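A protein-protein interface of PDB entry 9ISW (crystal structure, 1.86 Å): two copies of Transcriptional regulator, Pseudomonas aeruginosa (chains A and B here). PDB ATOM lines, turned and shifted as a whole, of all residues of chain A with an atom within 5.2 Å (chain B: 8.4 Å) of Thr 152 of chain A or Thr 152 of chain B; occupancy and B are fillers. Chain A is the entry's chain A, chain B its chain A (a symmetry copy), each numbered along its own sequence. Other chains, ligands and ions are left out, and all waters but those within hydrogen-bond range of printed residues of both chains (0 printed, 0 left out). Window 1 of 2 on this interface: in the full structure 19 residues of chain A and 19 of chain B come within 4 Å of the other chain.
The backbone carbonyl oxygen of Tyr 148 of chain B lies within hydrogen-bond range of the side-chain hydroxyl of Thr 152 of chain B, 2.7 Å away.
The side-chain amide oxygen (OD1) of Asn 146 of chain B is in hydrogen-bond range of the backbone NH (N) of Leu 149 of chain B, at 2.9 Å.
ND2 of Asn 155 of chain A lies close to O of Glu 151 of chain A.
OD1 of Asn 146 of chain B sits at hydrogen-bond distance from N of Tyr 148 of chain B (3.1 Å).
The backbone carbonyl oxygen (O) of Tyr 148 of chain A lies within hydrogen-bond range of the side-chain hydroxyl (OG1) of Thr 152 of chain A, 2.7 Å away.
Among the printed residues, merely in contact across the chains: Leu 85 of chain A with Leu 89 of chain B (3.5 Å), Leu 85 of chain A with Tyr 148 of chain B (3.8 Å), Leu 85 of chain A with Leu 149 of chain B (3.8 Å), Leu 85 of chain A with Thr 152 of chain B (3.96 Å), Leu 89 of chain A with Leu 85 of chain B (3.5 Å), Tyr 148 of chain A with His 59 of chain B (3.3 Å), Tyr 148 of chain A with Leu 82 of chain B (3.6 Å), Tyr 148 of chain A with Leu 85 of chain B (3.8 Å), Tyr 148 of chain A with Leu 156 of chain B (3.6 Å), Leu 149 of chain A with Leu 85 of chain B (3.8 Å), Glu 151 of chain A with Arg 57 of chain B (3.9 Å), Glu 151 of chain A with His 59 of chain B (3.0 Å), Thr 152 of chain A with Leu 85 of chain B (3.96 Å), Thr 152 of chain A with Thr 152 of chain B (3.6 Å) and Leu 156 of chain A with Tyr 148 of chain B (3.6 Å).
Thr 152 of chain B touches just these residues of chain A: Leu 85 (3.96 Å) and Thr 152 (3.6 Å).
Printed residues of chain A within 4 Å of Leu 89 of chain B: Leu 85 (3.5 Å).
Printed residues of chain A within 4 Å of Tyr 148 of chain B: Leu 85 and Leu 156.
Asn 155 of chain B touches none of the printed residues of chain A.
Asn 146 of chain B touches none of the printed residues of chain A.
The nearest printed residue of chain B that does not touch Leu 89 of chain A is Leu 89 of chain B (4.6 Å).
Of the 22 printed residues of chain B, 9 touch a printed residue of chain A.
Hydrophobic or aromatic side chains of chain A that line the printed part of chain B: Leu 85, Leu 89, Tyr 148 and Leu 156.
Among the printed residues, no Asp or Glu carboxylate lies within 4 Å of a Lys or Arg side-chain nitrogen of the other chain.
Leu 85 of chain A touches Tyr 148 of chain B, and with the chains exchanged Tyr 148 of chain A touches Leu 85 of chain B.
Leu 85 of chain A touches Thr 152 of chain B, and with the chains exchanged Thr 152 of chain A touches Leu 85 of chain B.
Tyr 148 of chain A touches Leu 156 of chain B, and with the chains exchanged Leu 156 of chain A touches Tyr 148 of chain B.
Thr 152 of chain A touches its own counterpart, Thr 152 of chain B.
12 positions are printed for both chains.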
ATOM      1  N   LEU A  85      -1.267 -13.548  35.291  1.00  0.00           N
ATOM      2  CA  LEU A  85      -0.683 -14.729  34.662  1.00  0.00           C
ATOM      3  C   LEU A  85       0.187 -15.518  35.632  1.00  0.00           C
ATOM      4  O   LEU A  85       0.044 -16.743  35.758  1.00  0.00           O
ATOM      5  CB  LEU A  85       0.135 -14.300  33.440  1.00  0.00           C
ATOM      6  CG  LEU A  85       0.958 -15.378  32.737  1.00  0.00           C
ATOM      7  CD1 LEU A  85       0.062 -16.492  32.220  1.00  0.00           C
ATOM      8  CD2 LEU A  85       1.751 -14.759  31.567  1.00  0.00           C
ATOM      9  N   LEU A  89       0.425 -19.632  36.934  1.00  0.00           N
ATOM     10  CA  LEU A  89       1.600 -20.485  36.747  1.00  0.00           C
ATOM     11  C   LEU A  89       2.128 -21.014  38.078  1.00  0.00           C
ATOM     12  O   LEU A  89       2.570 -22.171  38.165  1.00  0.00           O
ATOM     13  CB  LEU A  89       2.687 -19.701  36.025  1.00  0.00           C
ATOM     14  CG  LEU A  89       2.267 -19.007  34.731  1.00  0.00           C
ATOM     15  CD1 LEU A  89       3.441 -18.217  34.166  1.00  0.00           C
ATOM     16  CD2 LEU A  89       1.780 -20.035  33.723  1.00  0.00           C
ATOM     17  N   PRO A 147       8.157 -28.843  30.653  1.00  0.00           N
ATOM     18  CA  PRO A 147       9.058 -27.899  29.974  1.00  0.00           C
ATOM     19  C   PRO A 147       8.355 -26.628  29.549  1.00  0.00           C
ATOM     20  O   PRO A 147       8.973 -25.560  29.554  1.00  0.00           O
ATOM     21  CB  PRO A 147       9.558 -28.704  28.768  1.00  0.00           C
ATOM     22  CG  PRO A 147       8.480 -29.691  28.499  1.00  0.00           C
ATOM     23  CD  PRO A 147       7.884 -30.040  29.839  1.00  0.00           C
ATOM     24  N   TYR A 148       7.070 -26.707  29.203  1.00  0.00           N
ATOM     25  CA  TYR A 148       6.355 -25.513  28.765  1.00  0.00           C
ATOM     26  C   TYR A 148       6.188 -24.541  29.918  1.00  0.00           C
ATOM     27  O   TYR A 148       6.421 -23.336  29.774  1.00  0.00           O
ATOM     28  CB  TYR A 148       4.997 -25.908  28.205  1.00  0.00           C
ATOM     29  CG  TYR A 148       5.132 -26.896  27.067  1.00  0.00           C
ATOM     30  CD1 TYR A 148       5.647 -26.493  25.840  1.00  0.00           C
ATOM     31  CD2 TYR A 148       4.769 -28.230  27.225  1.00  0.00           C
ATOM     32  CE1 TYR A 148       5.790 -27.387  24.784  1.00  0.00           C
ATOM     33  CE2 TYR A 148       4.917 -29.140  26.153  1.00  0.00           C
ATOM     34  CZ  TYR A 148       5.421 -28.701  24.950  1.00  0.00           C
ATOM     35  OH  TYR A 148       5.555 -29.575  23.875  1.00  0.00           O
ATOM     36  N   LEU A 149       5.766 -25.064  31.065  1.00  0.00           N
ATOM     37  CA  LEU A 149       5.604 -24.257  32.267  1.00  0.00           C
ATOM     38  C   LEU A 149       6.938 -23.705  32.746  1.00  0.00           C
ATOM     39  O   LEU A 149       7.037 -22.528  33.103  1.00  0.00           O
ATOM     40  CB  LEU A 149       4.949 -25.120  33.351  1.00  0.00           C
ATOM     41  CG  LEU A 149       4.772 -24.529  34.745  1.00  0.00           C
ATOM     42  CD1 LEU A 149       3.871 -23.316  34.663  1.00  0.00           C
ATOM     43  CD2 LEU A 149       4.163 -25.595  35.644  1.00  0.00           C
ATOM     44  N   GLN A 150       7.982 -24.542  32.761  1.00  0.00           N
ATOM     45  CA  GLN A 150       9.293 -24.085  33.218  1.00  0.00           C
ATOM     46  C   GLN A 150       9.814 -22.949  32.350  1.00  0.00           C
ATOM     47  O   GLN A 150      10.276 -21.913  32.854  1.00  0.00           O
ATOM     48  CB  GLN A 150      10.281 -25.256  33.197  1.00  0.00           C
ATOM     49  CG  GLN A 150      11.666 -24.883  33.650  1.00  0.00           C
ATOM     50  CD  GLN A 150      12.521 -26.112  33.893  1.00  0.00           C
ATOM     51  OE1 GLN A 150      11.998 -27.207  34.090  1.00  0.00           O
ATOM     52  NE2 GLN A 150      13.831 -25.941  33.866  1.00  0.00           N
ATOM     53  N   GLU A 151       9.772 -23.131  31.034  1.00  0.00           N
ATOM     54  CA  GLU A 151      10.311 -22.096  30.161  1.00  0.00           C
ATOM     55  C   GLU A 151       9.485 -20.820  30.251  1.00  0.00           C
ATOM     56  O   GLU A 151      10.036 -19.714  30.218  1.00  0.00           O
ATOM     57  CB  GLU A 151      10.394 -22.630  28.736  1.00  0.00           C
ATOM     58  CG  GLU A 151      11.359 -23.819  28.695  1.00  0.00           C
ATOM     59  CD  GLU A 151      11.804 -24.215  27.300  1.00  0.00           C
ATOM     60  OE1 GLU A 151      11.461 -23.501  26.330  1.00  0.00           O
ATOM     61  OE2 GLU A 151      12.504 -25.251  27.185  1.00  0.00           O
ATOM     62  N   THR A 152       8.158 -20.954  30.380  1.00  0.00           N
ATOM     63  CA  THR A 152       7.314 -19.771  30.543  1.00  0.00           C
ATOM     64  C   THR A 152       7.692 -18.999  31.806  1.00  0.00           C
ATOM     65  O   THR A 152       7.911 -17.779  31.765  1.00  0.00           O
ATOM     66  CB  THR A 152       5.836 -20.185  30.575  1.00  0.00           C
ATOM     67  OG1 THR A 152       5.482 -20.813  29.335  1.00  0.00           O
ATOM     68  CG2 THR A 152       4.929 -18.964  30.787  1.00  0.00           C
ATOM     69  N   VAL A 153       7.803 -19.697  32.938  1.00  0.00           N
ATOM     70  CA  VAL A 153       8.157 -19.029  34.189  1.00  0.00           C
ATOM     71  C   VAL A 153       9.556 -18.416  34.099  1.00  0.00           C
ATOM     72  O   VAL A 153       9.771 -17.262  34.489  1.00  0.00           O
ATOM     73  CB  VAL A 153       8.025 -20.008  35.369  1.00  0.00           C
ATOM     74  CG1 VAL A 153       8.643 -19.428  36.635  1.00  0.00           C
ATOM     75  CG2 VAL A 153       6.534 -20.320  35.588  1.00  0.00           C
ATOM     76  N   GLU A 154      10.522 -19.166  33.566  1.00  0.00           N
ATOM     77  CA  GLU A 154      11.877 -18.619  33.430  1.00  0.00           C
ATOM     78  C   GLU A 154      11.878 -17.344  32.584  1.00  0.00           C
ATOM     79  O   GLU A 154      12.562 -16.365  32.918  1.00  0.00           O
ATOM     80  CB  GLU A 154      12.811 -19.685  32.835  1.00  0.00           C
ATOM     81  CG  GLU A 154      13.139 -20.814  33.817  1.00  0.00           C
ATOM     82  CD  GLU A 154      13.924 -21.979  33.201  1.00  0.00           C
ATOM     83  OE1 GLU A 154      13.956 -22.112  31.957  1.00  0.00           O
ATOM     84  OE2 GLU A 154      14.520 -22.771  33.970  1.00  0.00           O
ATOM     85  N   ASN A 155      11.088 -17.318  31.512  1.00  0.00           N
ATOM     86  CA  ASN A 155      11.055 -16.143  30.643  1.00  0.00           C
ATOM     87  C   ASN A 155      10.405 -14.939  31.312  1.00  0.00           C
ATOM     88  O   ASN A 155      10.653 -13.807  30.885  1.00  0.00           O
ATOM     89  CB  ASN A 155      10.297 -16.451  29.360  1.00  0.00           C
ATOM     90  CG  ASN A 155      11.079 -17.330  28.417  1.00  0.00           C
ATOM     91  OD1 ASN A 155      12.292 -17.475  28.546  1.00  0.00           O
ATOM     92  ND2 ASN A 155      10.386 -17.913  27.443  1.00  0.00           N
ATOM     93  N   LEU A 156       9.545 -15.161  32.311  1.00  0.00           N
ATOM     94  CA  LEU A 156       8.868 -14.083  33.029  1.00  0.00           C
ATOM     95  C   LEU A 156       9.592 -13.672  34.304  1.00  0.00           C
ATOM     96  O   LEU A 156       9.223 -12.660  34.910  1.00  0.00           O
ATOM     97  CB  LEU A 156       7.433 -14.498  33.386  1.00  0.00           C
ATOM     98  CG  LEU A 156       6.501 -14.746  32.201  1.00  0.00           C
ATOM     99  CD1 LEU A 156       5.204 -15.392  32.642  1.00  0.00           C
ATOM    100  CD2 LEU A 156       6.230 -13.438  31.453  1.00  0.00           C
ATOM    101  N   ARG B  57      13.212 -23.099  20.554  1.00  0.00           N
ATOM    102  CA  ARG B  57      12.535 -22.295  21.564  1.00  0.00           C
ATOM    103  C   ARG B  57      11.043 -22.617  21.626  1.00  0.00           C
ATOM    104  O   ARG B  57      10.437 -22.579  22.706  1.00  0.00           O
ATOM    105  CB  ARG B  57      12.761 -20.814  21.262  1.00  0.00           C
ATOM    106  CG  ARG B  57      12.165 -19.838  22.264  1.00  0.00           C
ATOM    107  CD  ARG B  57      12.702 -18.423  22.022  1.00  0.00           C
ATOM    108  NE  ARG B  57      11.991 -17.735  20.941  1.00  0.00           N
ATOM    109  CZ  ARG B  57      12.587 -17.148  19.905  1.00  0.00           C
ATOM    110  NH1 ARG B  57      13.914 -17.165  19.798  1.00  0.00           N
ATOM    111  NH2 ARG B  57      11.859 -16.545  18.970  1.00  0.00           N
ATOM    112  N   ARG B  58      10.441 -22.954  20.487  1.00  0.00           N
ATOM    113  CA  ARG B  58       9.022 -23.306  20.398  1.00  0.00           C
ATOM    114  C   ARG B  58       8.775 -24.794  20.595  1.00  0.00           C
ATOM    115  O   ARG B  58       7.668 -25.271  20.306  1.00  0.00           O
ATOM    116  CB  ARG B  58       8.441 -22.891  19.041  1.00  0.00           C
ATOM    117  CG  ARG B  58       8.697 -21.459  18.639  1.00  0.00           C
ATOM    118  CD  ARG B  58       7.947 -20.466  19.484  1.00  0.00           C
ATOM    119  NE  ARG B  58       8.352 -19.110  19.111  1.00  0.00           N
ATOM    120  CZ  ARG B  58       7.688 -18.332  18.260  1.00  0.00           C
ATOM    121  NH1 ARG B  58       6.557 -18.757  17.704  1.00  0.00           N
ATOM    122  NH2 ARG B  58       8.146 -17.118  17.972  1.00  0.00           N
ATOM    123  N   HIS B  59       9.797 -25.540  21.019  1.00  0.00           N
ATOM    124  CA  HIS B  59       9.697 -26.940  21.425  1.00  0.00           C
ATOM    125  C   HIS B  59       9.487 -27.905  20.263  1.00  0.00           C
ATOM    126  O   HIS B  59       9.155 -29.074  20.492  1.00  0.00           O
ATOM    127  CB  HIS B  59       8.584 -27.141  22.457  1.00  0.00           C
ATOM    128  CG  HIS B  59       8.615 -26.155  23.582  1.00  0.00           C
ATOM    129  ND1 HIS B  59       9.351 -26.363  24.725  1.00  0.00           N
ATOM    130  CD2 HIS B  59       7.990 -24.964  23.747  1.00  0.00           C
ATOM    131  CE1 HIS B  59       9.182 -25.342  25.548  1.00  0.00           C
ATOM    132  NE2 HIS B  59       8.362 -24.479  24.978  1.00  0.00           N
ATOM    133  N   LEU B  82       1.527 -29.635  28.387  1.00  0.00           N
ATOM    134  CA  LEU B  82       1.087 -28.565  27.496  1.00  0.00           C
ATOM    135  C   LEU B  82      -0.380 -28.234  27.726  1.00  0.00           C
ATOM    136  O   LEU B  82      -0.759 -27.058  27.830  1.00  0.00           O
ATOM    137  CB  LEU B  82       1.326 -28.990  26.051  1.00  0.00           C
ATOM    138  CG  LEU B  82       0.933 -28.002  24.966  1.00  0.00           C
ATOM    139  CD1 LEU B  82       1.752 -26.725  25.106  1.00  0.00           C
ATOM    140  CD2 LEU B  82       1.168 -28.658  23.623  1.00  0.00           C
ATOM    141  N   LEU B  85      -1.196 -26.386  31.019  1.00  0.00           N
ATOM    142  CA  LEU B  85      -0.851 -24.969  30.954  1.00  0.00           C
ATOM    143  C   LEU B  85      -1.790 -24.198  30.035  1.00  0.00           C
ATOM    144  O   LEU B  85      -2.323 -23.144  30.415  1.00  0.00           O
ATOM    145  CB  LEU B  85       0.599 -24.821  30.480  1.00  0.00           C
ATOM    146  CG  LEU B  85       1.099 -23.406  30.194  1.00  0.00           C
ATOM    147  CD1 LEU B  85       1.019 -22.540  31.441  1.00  0.00           C
ATOM    148  CD2 LEU B  85       2.554 -23.453  29.683  1.00  0.00           C
ATOM    149  N   ILE B  86      -1.980 -24.685  28.806  1.00  0.00           N
ATOM    150  CA  ILE B  86      -2.721 -23.897  27.823  1.00  0.00           C
ATOM    151  C   ILE B  86      -4.161 -23.683  28.259  1.00  0.00           C
ATOM    152  O   ILE B  86      -4.757 -22.635  27.965  1.00  0.00           O
ATOM    153  CB  ILE B  86      -2.628 -24.556  26.426  1.00  0.00           C
ATOM    154  CG1 ILE B  86      -2.955 -23.543  25.341  1.00  0.00           C
ATOM    155  CG2 ILE B  86      -3.582 -25.730  26.305  1.00  0.00           C
ATOM    156  CD1 ILE B  86      -1.789 -22.637  24.968  1.00  0.00           C
ATOM    157  N   LEU B  89      -4.222 -20.641  30.374  1.00  0.00           N
ATOM    158  CA  LEU B  89      -4.045 -19.445  29.551  1.00  0.00           C
ATOM    159  C   LEU B  89      -5.314 -19.104  28.774  1.00  0.00           C
ATOM    160  O   LEU B  89      -5.655 -17.922  28.610  1.00  0.00           O
ATOM    161  CB  LEU B  89      -2.884 -19.656  28.591  1.00  0.00           C
ATOM    162  CG  LEU B  89      -1.572 -20.123  29.218  1.00  0.00           C
ATOM    163  CD1 LEU B  89      -0.532 -20.351  28.127  1.00  0.00           C
ATOM    164  CD2 LEU B  89      -1.078 -19.094  30.221  1.00  0.00           C
ATOM    165  N   PHE B 141      -6.791 -11.373  21.873  1.00  0.00           N
ATOM    166  CA  PHE B 141      -5.703 -10.549  22.415  1.00  0.00           C
ATOM    167  C   PHE B 141      -6.083  -9.095  22.660  1.00  0.00           C
ATOM    168  O   PHE B 141      -5.701  -8.556  23.722  1.00  0.00           O
ATOM    169  CB  PHE B 141      -4.479 -10.630  21.490  1.00  0.00           C
ATOM    170  CG  PHE B 141      -3.813 -11.987  21.473  1.00  0.00           C
ATOM    171  CD1 PHE B 141      -3.884 -12.826  22.574  1.00  0.00           C
ATOM    172  CD2 PHE B 141      -3.118 -12.419  20.351  1.00  0.00           C
ATOM    173  CE1 PHE B 141      -3.262 -14.078  22.566  1.00  0.00           C
ATOM    174  CE2 PHE B 141      -2.499 -13.672  20.330  1.00  0.00           C
ATOM    175  CZ  PHE B 141      -2.575 -14.498  21.440  1.00  0.00           C
ATOM    176  N   ASN B 146      -2.741  -7.883  27.221  1.00  0.00           N
ATOM    177  CA  ASN B 146      -1.842  -8.518  28.180  1.00  0.00           C
ATOM    178  C   ASN B 146      -0.630  -9.023  27.410  1.00  0.00           C
ATOM    179  O   ASN B 146      -0.677 -10.115  26.821  1.00  0.00           O
ATOM    180  CB  ASN B 146      -2.563  -9.659  28.904  1.00  0.00           C
ATOM    181  CG  ASN B 146      -1.718 -10.303  29.966  1.00  0.00           C
ATOM    182  OD1 ASN B 146      -0.499 -10.346  29.856  1.00  0.00           O
ATOM    183  ND2 ASN B 146      -2.373 -10.841  31.007  1.00  0.00           N
ATOM    184  N   PRO B 147       0.467  -8.271  27.368  1.00  0.00           N
ATOM    185  CA  PRO B 147       1.597  -8.698  26.528  1.00  0.00           C
ATOM    186  C   PRO B 147       2.223  -9.988  27.010  1.00  0.00           C
ATOM    187  O   PRO B 147       2.696 -10.779  26.190  1.00  0.00           O
ATOM    188  CB  PRO B 147       2.571  -7.517  26.632  1.00  0.00           C
ATOM    189  CG  PRO B 147       2.260  -6.884  27.940  1.00  0.00           C
ATOM    190  CD  PRO B 147       0.778  -7.064  28.153  1.00  0.00           C
ATOM    191  N   TYR B 148       2.219 -10.237  28.320  1.00  0.00           N
ATOM    192  CA  TYR B 148       2.831 -11.457  28.835  1.00  0.00           C
ATOM    193  C   TYR B 148       2.035 -12.674  28.402  1.00  0.00           C
ATOM    194  O   TYR B 148       2.600 -13.677  27.950  1.00  0.00           O
ATOM    195  CB  TYR B 148       2.909 -11.388  30.353  1.00  0.00           C
ATOM    196  CG  TYR B 148       3.678 -10.170  30.814  1.00  0.00           C
ATOM    197  CD1 TYR B 148       5.054 -10.092  30.628  1.00  0.00           C
ATOM    198  CD2 TYR B 148       3.031  -9.093  31.411  1.00  0.00           C
ATOM    199  CE1 TYR B 148       5.779  -8.977  31.035  1.00  0.00           C
ATOM    200  CE2 TYR B 148       3.767  -7.958  31.823  1.00  0.00           C
ATOM    201  CZ  TYR B 148       5.129  -7.922  31.631  1.00  0.00           C
ATOM    202  OH  TYR B 148       5.877  -6.824  32.046  1.00  0.00           O
ATOM    203  N   LEU B 149       0.718 -12.594  28.557  1.00  0.00           N
ATOM    204  CA  LEU B 149      -0.174 -13.669  28.142  1.00  0.00           C
ATOM    205  C   LEU B 149      -0.133 -13.871  26.635  1.00  0.00           C
ATOM    206  O   LEU B 149      -0.070 -15.007  26.157  1.00  0.00           O
ATOM    207  CB  LEU B 149      -1.595 -13.334  28.610  1.00  0.00           C
ATOM    208  CG  LEU B 149      -2.735 -14.260  28.200  1.00  0.00           C
ATOM    209  CD1 LEU B 149      -2.487 -15.639  28.771  1.00  0.00           C
ATOM    210  CD2 LEU B 149      -4.038 -13.681  28.731  1.00  0.00           C
ATOM    211  N   GLN B 150      -0.168 -12.777  25.865  1.00  0.00           N
ATOM    212  CA  GLN B 150      -0.141 -12.894  24.408  1.00  0.00           C
ATOM    213  C   GLN B 150       1.135 -13.573  23.933  1.00  0.00           C
ATOM    214  O   GLN B 150       1.103 -14.500  23.107  1.00  0.00           O
ATOM    215  CB  GLN B 150      -0.260 -11.502  23.779  1.00  0.00           C
ATOM    216  CG  GLN B 150      -0.240 -11.518  22.275  1.00  0.00           C
ATOM    217  CD  GLN B 150      -0.650 -10.175  21.700  1.00  0.00           C
ATOM    218  OE1 GLN B 150      -1.296  -9.378  22.377  1.00  0.00           O
ATOM    219  NE2 GLN B 150      -0.268  -9.915  20.462  1.00  0.00           N
ATOM    220  N   GLU B 151       2.280 -13.111  24.423  1.00  0.00           N
ATOM    221  CA  GLU B 151       3.533 -13.689  23.957  1.00  0.00           C
ATOM    222  C   GLU B 151       3.658 -15.143  24.391  1.00  0.00           C
ATOM    223  O   GLU B 151       4.163 -15.981  23.634  1.00  0.00           O
ATOM    224  CB  GLU B 151       4.698 -12.838  24.449  1.00  0.00           C
ATOM    225  CG  GLU B 151       4.586 -11.431  23.852  1.00  0.00           C
ATOM    226  CD  GLU B 151       5.849 -10.601  23.969  1.00  0.00           C
ATOM    227  OE1 GLU B 151       6.888 -11.138  24.420  1.00  0.00           O
ATOM    228  OE2 GLU B 151       5.793  -9.402  23.603  1.00  0.00           O
ATOM    229  N   THR B 152       3.191 -15.466  25.604  1.00  0.00           N
ATOM    230  CA  THR B 152       3.215 -16.858  26.052  1.00  0.00           C
ATOM    231  C   THR B 152       2.382 -17.745  25.131  1.00  0.00           C
ATOM    232  O   THR B 152       2.853 -18.790  24.656  1.00  0.00           O
ATOM    233  CB  THR B 152       2.713 -16.947  27.501  1.00  0.00           C
ATOM    234  OG1 THR B 152       3.577 -16.189  28.360  1.00  0.00           O
ATOM    235  CG2 THR B 152       2.691 -18.404  27.984  1.00  0.00           C
ATOM    236  N   VAL B 153       1.146 -17.333  24.839  1.00  0.00           N
ATOM    237  CA  VAL B 153       0.285 -18.130  23.967  1.00  0.00           C
ATOM    238  C   VAL B 153       0.884 -18.235  22.564  1.00  0.00           C
ATOM    239  O   VAL B 153       0.937 -19.321  21.973  1.00  0.00           O
ATOM    240  CB  VAL B 153      -1.139 -17.547  23.951  1.00  0.00           C
ATOM    241  CG1 VAL B 153      -1.980 -18.184  22.851  1.00  0.00           C
ATOM    242  CG2 VAL B 153      -1.784 -17.779  25.328  1.00  0.00           C
ATOM    243  N   GLU B 154       1.364 -17.117  22.016  1.00  0.00           N
ATOM    244  CA  GLU B 154       1.975 -17.164  20.682  1.00  0.00           C
ATOM    245  C   GLU B 154       3.154 -18.139  20.645  1.00  0.00           C
ATOM    246  O   GLU B 154       3.311 -18.904  19.682  1.00  0.00           O
ATOM    247  CB  GLU B 154       2.405 -15.752  20.257  1.00  0.00           C
ATOM    248  CG  GLU B 154       1.223 -14.839  19.914  1.00  0.00           C
ATOM    249  CD  GLU B 154       1.607 -13.377  19.655  1.00  0.00           C
ATOM    250  OE1 GLU B 154       2.719 -12.953  20.045  1.00  0.00           O
ATOM    251  OE2 GLU B 154       0.788 -12.641  19.052  1.00  0.00           O
ATOM    252  N   ASN B 155       3.966 -18.159  21.701  1.00  0.00           N
ATOM    253  CA  ASN B 155       5.127 -19.047  21.727  1.00  0.00           C
ATOM    254  C   ASN B 155       4.738 -20.516  21.835  1.00  0.00           C
ATOM    255  O   ASN B 155       5.543 -21.380  21.474  1.00  0.00           O
ATOM    256  CB  ASN B 155       6.036 -18.700  22.896  1.00  0.00           C
ATOM    257  CG  ASN B 155       6.811 -17.426  22.676  1.00  0.00           C
ATOM    258  OD1 ASN B 155       6.928 -16.943  21.552  1.00  0.00           O
ATOM    259  ND2 ASN B 155       7.365 -16.879  23.754  1.00  0.00           N
ATOM    260  N   LEU B 156       3.549 -20.815  22.367  1.00  0.00           N
ATOM    261  CA  LEU B 156       3.068 -22.188  22.515  1.00  0.00           C
ATOM    262  C   LEU B 156       2.190 -22.638  21.355  1.00  0.00           C
ATOM    263  O   LEU B 156       1.864 -23.827  21.269  1.00  0.00           O
ATOM    264  CB  LEU B 156       2.278 -22.339  23.823  1.00  0.00           C
ATOM    265  CG  LEU B 156       3.075 -22.125  25.109  1.00  0.00           C
ATOM    266  CD1 LEU B 156       2.166 -22.041  26.316  1.00  0.00           C
ATOM    267  CD2 LEU B 156       4.111 -23.239  25.284  1.00  0.00           C
ATOM    268  N   LEU B 157       1.794 -21.726  20.468  1.00  0.00           N
ATOM    269  CA  LEU B 157       0.862 -22.096  19.405  1.00  0.00           C
ATOM    270  C   LEU B 157       1.403 -23.195  18.491  1.00  0.00           C
ATOM    271  O   LEU B 157       0.621 -24.083  18.122  1.00  0.00           O
ATOM    272  CB  LEU B 157       0.481 -20.855  18.585  1.00  0.00           C
ATOM    273  CG  LEU B 157      -0.456 -19.807  19.189  1.00  0.00           C
ATOM    274  CD1 LEU B 157      -0.960 -18.858  18.097  1.00  0.00           C
ATOM    275  CD2 LEU B 157      -1.615 -20.463  19.903  1.00  0.00           C
ATOM    276  N   PRO B 158       2.677 -23.188  18.080  1.00  0.00           N
ATOM    277  CA  PRO B 158       3.159 -24.314  17.247  1.00  0.00           C
ATOM    278  C   PRO B 158       3.026 -25.669  17.929  1.00  0.00           C
ATOM    279  O   PRO B 158       2.554 -26.628  17.302  1.00  0.00           O
ATOM    280  CB  PRO B 158       4.625 -23.940  16.980  1.00  0.00           C
ATOM    281  CG  PRO B 158       4.644 -22.433  17.076  1.00  0.00           C
ATOM    282  CD  PRO B 158       3.676 -22.108  18.171  1.00  0.00           C
ATOM    283  N   VAL B 160       0.977 -26.550  20.458  1.00  0.00           N
ATOM    284  CA  VAL B 160      -0.458 -26.829  20.547  1.00  0.00           C
ATOM    285  C   VAL B 160      -0.995 -27.273  19.195  1.00  0.00           C
ATOM    286  O   VAL B 160      -1.772 -28.228  19.091  1.00  0.00           O
ATOM    287  CB  VAL B 160      -1.203 -25.577  21.049  1.00  0.00           C
ATOM    288  CG1 VAL B 160      -2.707 -25.724  20.848  1.00  0.00           C
ATOM    289  CG2 VAL B 160      -0.850 -25.292  22.515  1.00  0.00           C
